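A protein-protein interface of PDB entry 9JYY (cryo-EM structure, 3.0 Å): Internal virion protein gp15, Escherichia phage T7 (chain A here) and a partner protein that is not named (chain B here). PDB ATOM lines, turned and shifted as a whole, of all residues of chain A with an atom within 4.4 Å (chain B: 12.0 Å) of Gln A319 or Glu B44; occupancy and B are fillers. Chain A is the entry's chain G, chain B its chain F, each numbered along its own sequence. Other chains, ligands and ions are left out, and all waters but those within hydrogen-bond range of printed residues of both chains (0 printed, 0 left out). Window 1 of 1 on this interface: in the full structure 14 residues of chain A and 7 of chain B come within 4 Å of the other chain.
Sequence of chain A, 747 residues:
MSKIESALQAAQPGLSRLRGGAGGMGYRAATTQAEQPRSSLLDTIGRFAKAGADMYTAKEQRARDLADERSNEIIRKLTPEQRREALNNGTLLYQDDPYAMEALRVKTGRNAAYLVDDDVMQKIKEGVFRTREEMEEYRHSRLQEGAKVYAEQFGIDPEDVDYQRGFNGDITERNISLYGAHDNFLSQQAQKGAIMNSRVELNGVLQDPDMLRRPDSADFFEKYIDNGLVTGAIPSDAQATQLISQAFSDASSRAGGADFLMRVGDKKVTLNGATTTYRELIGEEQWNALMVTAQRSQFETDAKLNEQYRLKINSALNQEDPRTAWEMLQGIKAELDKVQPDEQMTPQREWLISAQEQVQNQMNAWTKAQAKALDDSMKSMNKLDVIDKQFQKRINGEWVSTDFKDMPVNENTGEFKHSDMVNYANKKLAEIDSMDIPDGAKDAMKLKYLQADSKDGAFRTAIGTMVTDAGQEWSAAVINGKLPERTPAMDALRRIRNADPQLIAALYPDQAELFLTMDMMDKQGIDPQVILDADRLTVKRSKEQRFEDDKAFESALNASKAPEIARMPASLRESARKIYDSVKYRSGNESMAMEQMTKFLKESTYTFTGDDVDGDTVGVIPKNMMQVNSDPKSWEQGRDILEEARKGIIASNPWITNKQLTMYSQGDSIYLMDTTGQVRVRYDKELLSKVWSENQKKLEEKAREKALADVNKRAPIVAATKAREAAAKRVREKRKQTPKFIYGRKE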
ATOM      1  N   SER A 315      31.634   6.895 -12.620  1.00  0.00           N
ATOM      2  CA  SER A 315      31.599   5.984 -13.751  1.00  0.00           C
ATOM      3  C   SER A 315      30.187   5.483 -13.998  1.00  0.00           C
ATOM      4  O   SER A 315      29.770   5.320 -15.148  1.00  0.00           O
ATOM      5  CB  SER A 315      32.552   4.821 -13.499  1.00  0.00           C
ATOM      6  OG  SER A 315      32.432   3.875 -14.530  1.00  0.00           O
ATOM      7  N   ALA A 316      29.441   5.215 -12.926  1.00  0.00           N
ATOM      8  CA  ALA A 316      28.021   4.932 -13.093  1.00  0.00           C
ATOM      9  C   ALA A 316      27.282   6.151 -13.626  1.00  0.00           C
ATOM     10  O   ALA A 316      26.432   6.029 -14.510  1.00  0.00           O
ATOM     11  CB  ALA A 316      27.409   4.471 -11.774  1.00  0.00           C
ATOM     12  N   LEU A 317      27.599   7.336 -13.109  1.00  0.00           N
ATOM     13  CA  LEU A 317      26.895   8.548 -13.514  1.00  0.00           C
ATOM     14  C   LEU A 317      27.100   8.902 -14.976  1.00  0.00           C
ATOM     15  O   LEU A 317      26.257   9.598 -15.548  1.00  0.00           O
ATOM     16  CB  LEU A 317      27.328   9.734 -12.655  1.00  0.00           C
ATOM     17  CG  LEU A 317      26.768   9.818 -11.239  1.00  0.00           C
ATOM     18  CD1 LEU A 317      27.430  10.948 -10.487  1.00  0.00           C
ATOM     19  CD2 LEU A 317      25.271  10.024 -11.296  1.00  0.00           C
ATOM     20  N   ASN A 318      28.193   8.456 -15.588  1.00  0.00           N
ATOM     21  CA  ASN A 318      28.517   8.801 -16.963  1.00  0.00           C
ATOM     22  C   ASN A 318      28.176   7.696 -17.949  1.00  0.00           C
ATOM     23  O   ASN A 318      28.778   7.630 -19.023  1.00  0.00           O
ATOM     24  CB  ASN A 318      29.994   9.160 -17.071  1.00  0.00           C
ATOM     25  CG  ASN A 318      30.307  10.487 -16.437  1.00  0.00           C
ATOM     26  OD1 ASN A 318      29.408  11.275 -16.153  1.00  0.00           O
ATOM     27  ND2 ASN A 318      31.577  10.732 -16.176  1.00  0.00           N
ATOM     28  N   GLN A 319      27.244   6.818 -17.602  1.00  0.00           N
ATOM     29  CA  GLN A 319      26.815   5.784 -18.529  1.00  0.00           C
ATOM     30  C   GLN A 319      26.003   6.386 -19.663  1.00  0.00           C
ATOM     31  O   GLN A 319      25.246   7.340 -19.477  1.00  0.00           O
ATOM     32  CB  GLN A 319      25.981   4.734 -17.809  1.00  0.00           C
ATOM     33  CG  GLN A 319      26.775   3.901 -16.860  1.00  0.00           C
ATOM     34  CD  GLN A 319      27.921   3.222 -17.552  1.00  0.00           C
ATOM     35  OE1 GLN A 319      27.743   2.612 -18.601  1.00  0.00           O
ATOM     36  NE2 GLN A 319      29.105   3.313 -16.968  1.00  0.00           N
ATOM     37  N   GLU A 320      26.165   5.815 -20.854  1.00  0.00           N
ATOM     38  CA  GLU A 320      25.404   6.305 -21.994  1.00  0.00           C
ATOM     39  C   GLU A 320      23.914   6.027 -21.827  1.00  0.00           C
ATOM     40  O   GLU A 320      23.082   6.899 -22.094  1.00  0.00           O
ATOM     41  CB  GLU A 320      25.927   5.687 -23.284  1.00  0.00           C
ATOM     42  CG  GLU A 320      25.199   6.198 -24.507  1.00  0.00           C
ATOM     43  CD  GLU A 320      25.423   7.685 -24.747  1.00  0.00           C
ATOM     44  OE1 GLU A 320      26.468   8.214 -24.314  1.00  0.00           O
ATOM     45  OE2 GLU A 320      24.549   8.324 -25.368  1.00  0.00           O
ATOM     46  N   ASP A 321      23.557   4.830 -21.371  1.00  0.00           N
ATOM     47  CA  ASP A 321      22.162   4.526 -21.110  1.00  0.00           C
ATOM     48  C   ASP A 321      21.885   4.662 -19.618  1.00  0.00           C
ATOM     49  O   ASP A 321      22.395   3.863 -18.824  1.00  0.00           O
ATOM     50  CB  ASP A 321      21.823   3.109 -21.590  1.00  0.00           C
ATOM     51  CG  ASP A 321      20.381   2.710 -21.301  1.00  0.00           C
ATOM     52  OD1 ASP A 321      19.540   3.603 -21.076  1.00  0.00           O
ATOM     53  OD2 ASP A 321      20.083   1.498 -21.301  1.00  0.00           O
ATOM     54  N   THR A 324      21.325   1.688 -17.276  1.00  0.00           N
ATOM     55  CA  THR A 324      22.532   1.009 -16.827  1.00  0.00           C
ATOM     56  C   THR A 324      23.165   1.748 -15.657  1.00  0.00           C
ATOM     57  O   THR A 324      23.693   1.124 -14.730  1.00  0.00           O
ATOM     58  CB  THR A 324      23.508   0.879 -17.996  1.00  0.00           C
ATOM     59  OG1 THR A 324      23.058  -0.155 -18.882  1.00  0.00           O
ATOM     60  CG2 THR A 324      24.894   0.534 -17.506  1.00  0.00           C
ATOM     61  N   ALA A 325      23.107   3.080 -15.671  1.00  0.00           N
ATOM     62  CA  ALA A 325      23.589   3.855 -14.533  1.00  0.00           C
ATOM     63  C   ALA A 325      22.821   3.499 -13.272  1.00  0.00           C
ATOM     64  O   ALA A 325      23.404   3.349 -12.194  1.00  0.00           O
ATOM     65  CB  ALA A 325      23.461   5.347 -14.830  1.00  0.00           C
ATOM     66  N   MET A 328      24.024   0.118 -12.005  1.00  0.00           N
ATOM     67  CA  MET A 328      25.326   0.221 -11.357  1.00  0.00           C
ATOM     68  C   MET A 328      25.210   0.878  -9.989  1.00  0.00           C
ATOM     69  O   MET A 328      25.890   0.478  -9.033  1.00  0.00           O
ATOM     70  CB  MET A 328      26.280   1.007 -12.248  1.00  0.00           C
ATOM     71  CG  MET A 328      26.629   0.305 -13.538  1.00  0.00           C
ATOM     72  SD  MET A 328      27.682   1.319 -14.576  1.00  0.00           S
ATOM     73  CE  MET A 328      29.212   1.285 -13.651  1.00  0.00           C
ATOM     74  N   ASP B  39      18.043   2.028 -28.651  1.00  0.00           N
ATOM     75  CA  ASP B  39      17.559   3.263 -28.062  1.00  0.00           C
ATOM     76  C   ASP B  39      18.215   4.452 -28.750  1.00  0.00           C
ATOM     77  O   ASP B  39      19.278   4.327 -29.360  1.00  0.00           O
ATOM     78  CB  ASP B  39      17.871   3.276 -26.573  1.00  0.00           C
ATOM     79  CG  ASP B  39      17.104   2.219 -25.820  1.00  0.00           C
ATOM     80  OD1 ASP B  39      15.996   1.860 -26.267  1.00  0.00           O
ATOM     81  OD2 ASP B  39      17.615   1.739 -24.788  1.00  0.00           O
ATOM     82  N   GLU B  40      17.576   5.615 -28.661  1.00  0.00           N
ATOM     83  CA  GLU B  40      18.156   6.788 -29.296  1.00  0.00           C
ATOM     84  C   GLU B  40      19.466   7.170 -28.630  1.00  0.00           C
ATOM     85  O   GLU B  40      19.575   7.201 -27.403  1.00  0.00           O
ATOM     86  CB  GLU B  40      17.240   8.004 -29.228  1.00  0.00           C
ATOM     87  CG  GLU B  40      17.862   9.158 -30.019  1.00  0.00           C
ATOM     88  CD  GLU B  40      17.162  10.481 -29.842  1.00  0.00           C
ATOM     89  OE1 GLU B  40      16.243  10.551 -29.012  1.00  0.00           O
ATOM     90  OE2 GLU B  40      17.544  11.455 -30.525  1.00  0.00           O
ATOM     91  N   THR B  41      20.454   7.495 -29.450  1.00  0.00           N
ATOM     92  CA  THR B  41      21.631   8.174 -28.948  1.00  0.00           C
ATOM     93  C   THR B  41      21.287   9.622 -28.635  1.00  0.00           C
ATOM     94  O   THR B  41      20.813  10.362 -29.502  1.00  0.00           O
ATOM     95  CB  THR B  41      22.746   8.108 -29.983  1.00  0.00           C
ATOM     96  OG1 THR B  41      22.216   8.486 -31.260  1.00  0.00           O
ATOM     97  CG2 THR B  41      23.314   6.695 -30.066  1.00  0.00           C
ATOM     98  N   ASP B  42      21.519  10.029 -27.390  1.00  0.00           N
ATOM     99  CA  ASP B  42      21.191  11.377 -26.948  1.00  0.00           C
ATOM    100  C   ASP B  42      22.438  12.107 -26.466  1.00  0.00           C
ATOM    101  O   ASP B  42      23.428  11.481 -26.075  1.00  0.00           O
ATOM    102  CB  ASP B  42      20.085  11.361 -25.864  1.00  0.00           C
ATOM    103  CG  ASP B  42      20.600  11.081 -24.447  1.00  0.00           C
ATOM    104  OD1 ASP B  42      21.755  10.664 -24.249  1.00  0.00           O
ATOM    105  OD2 ASP B  42      19.821  11.309 -23.502  1.00  0.00           O
ATOM    106  N   THR B  43      22.393  13.435 -26.534  1.00  0.00           N
ATOM    107  CA  THR B  43      23.511  14.239 -26.066  1.00  0.00           C
ATOM    108  C   THR B  43      23.626  14.133 -24.555  1.00  0.00           C
ATOM    109  O   THR B  43      22.622  14.131 -23.837  1.00  0.00           O
ATOM    110  CB  THR B  43      23.339  15.697 -26.484  1.00  0.00           C
ATOM    111  OG1 THR B  43      22.103  16.204 -25.964  1.00  0.00           O
ATOM    112  CG2 THR B  43      23.327  15.810 -27.996  1.00  0.00           C
ATOM    113  N   GLU B  44      24.862  14.036 -24.071  1.00  0.00           N
ATOM    114  CA  GLU B  44      25.145  13.792 -22.665  1.00  0.00           C
ATOM    115  C   GLU B  44      26.020  14.906 -22.113  1.00  0.00           C
ATOM    116  O   GLU B  44      26.976  15.333 -22.769  1.00  0.00           O
ATOM    117  CB  GLU B  44      25.832  12.439 -22.484  1.00  0.00           C
ATOM    118  CG  GLU B  44      25.779  11.899 -21.074  1.00  0.00           C
ATOM    119  CD  GLU B  44      26.301  10.482 -20.984  1.00  0.00           C
ATOM    120  OE1 GLU B  44      26.796   9.968 -22.007  1.00  0.00           O
ATOM    121  OE2 GLU B  44      26.222   9.884 -19.891  1.00  0.00           O
ATOM    122  N   GLY B  45      25.691  15.371 -20.914  1.00  0.00           N
ATOM    123  CA  GLY B  45      26.506  16.340 -20.191  1.00  0.00           C
ATOM    124  C   GLY B  45      27.176  15.662 -19.009  1.00  0.00           C
ATOM    125  O   GLY B  45      26.507  15.030 -18.190  1.00  0.00           O
ATOM    126  N   THR B  46      28.497  15.808 -18.927  1.00  0.00           N
ATOM    127  CA  THR B  46      29.275  15.091 -17.926  1.00  0.00           C
ATOM    128  C   THR B  46      28.834  15.480 -16.523  1.00  0.00           C
ATOM    129  O   THR B  46      28.728  16.665 -16.196  1.00  0.00           O
ATOM    130  CB  THR B  46      30.762  15.386 -18.106  1.00  0.00           C
ATOM    131  OG1 THR B  46      30.994  16.783 -17.905  1.00  0.00           O
ATOM    132  CG2 THR B  46      31.210  15.001 -19.503  1.00  0.00           C
ATOM    133  N   GLU B  47      28.594  14.475 -15.686  1.00  0.00           N
ATOM    134  CA  GLU B  47      28.045  14.676 -14.353  1.00  0.00           C
ATOM    135  C   GLU B  47      28.969  14.059 -13.317  1.00  0.00           C
ATOM    136  O   GLU B  47      29.491  12.958 -13.518  1.00  0.00           O
ATOM    137  CB  GLU B  47      26.644  14.076 -14.245  1.00  0.00           C
ATOM    138  CG  GLU B  47      25.612  14.794 -15.097  1.00  0.00           C
ATOM    139  CD  GLU B  47      24.232  14.177 -14.993  1.00  0.00           C
ATOM    140  OE1 GLU B  47      24.100  13.112 -14.355  1.00  0.00           O
ATOM    141  OE2 GLU B  47      23.274  14.759 -15.543  1.00  0.00           O
ATOM    142  N   VAL B  48      29.173  14.780 -12.218  1.00  0.00           N
ATOM    143  CA  VAL B  48      30.022  14.352 -11.116  1.00  0.00           C
ATOM    144  C   VAL B  48      29.222  14.482  -9.828  1.00  0.00           C
ATOM    145  O   VAL B  48      28.569  15.506  -9.602  1.00  0.00           O
ATOM    146  CB  VAL B  48      31.314  15.184 -11.044  1.00  0.00           C
ATOM    147  CG1 VAL B  48      32.175  14.744  -9.868  1.00  0.00           C
ATOM    148  CG2 VAL B  48      32.084  15.078 -12.351  1.00  0.00           C
ATOM    149  N   SER B  49      29.270  13.447  -8.995  1.00  0.00           N
ATOM    150  CA  SER B  49      28.558  13.444  -7.720  1.00  0.00           C
ATOM    151  C   SER B  49      28.978  14.607  -6.828  1.00  0.00           C
ATOM    152  O   SER B  49      30.142  15.005  -6.817  1.00  0.00           O
ATOM    153  CB  SER B  49      28.785  12.122  -6.988  1.00  0.00           C
ATOM    154  OG  SER B  49      30.165  11.845  -6.856  1.00  0.00           O
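The backbone carbonyl oxygen of Glu B47 lies close to the side-chain amide oxygen of Asn A318, 3.1 Å away. O of Gln A319 sits close to OE2 of Glu B44 (2.8 Å). OE2 of Glu A320 sits close to O of Asp B42 (3.4 Å). The side-chain carboxylate (OE1) of Glu B44 sits close to the side-chain carboxylate (OE1) of Glu A320 (2.9 Å).
The side-chain amide nitrogen (NE2) of Gln A319 is in hydrogen-bond range of the backbone carbonyl oxygen (O) of Ser A315, at 2.8 Å. NE2 of Gln A319 lies within hydrogen-bond range of SD of Met A328 (3.4 Å).
Among the printed residues, merely in contact across the chains: Leu A317 with Ser B49 (3.4 Å), Asn A318 with Glu B44 (3.5 Å) and Leu A317 with Glu B47 (3.98 Å).
Of chain B, only Glu B44 (2.8 Å) comes within 4 Å of Gln A319. Printed residues of chain A within 4 Å of Glu B44: Asn A318, Gln A319 and Glu A320. No residue of chain B comes within 4 Å of Ser A315. Glu A320 touches just these residues of chain B: Asp B42 and Glu B44. No residue of chain B comes within 4 Å of Asp A321. No residue of chain B comes within 4 Å of Thr A324. No residue of chain B comes within 4 Å of Ala A325. Of the printed residues of chain A, Ser B49 touches Leu A317. Of the printed residues of chain A, Asp B42 touches Glu A320. Thr B46 touches none of the printed residues of chain A.
Printed residues of chain B that touch a printed residue of chain A: Asp B42, Glu B44, Glu B47 and Ser B49. Of the 10 printed residues of chain A, 4 touch a printed residue of chain B. Hydrophobic or aromatic side chains of chain A that line the printed part of chain B: Leu A317.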
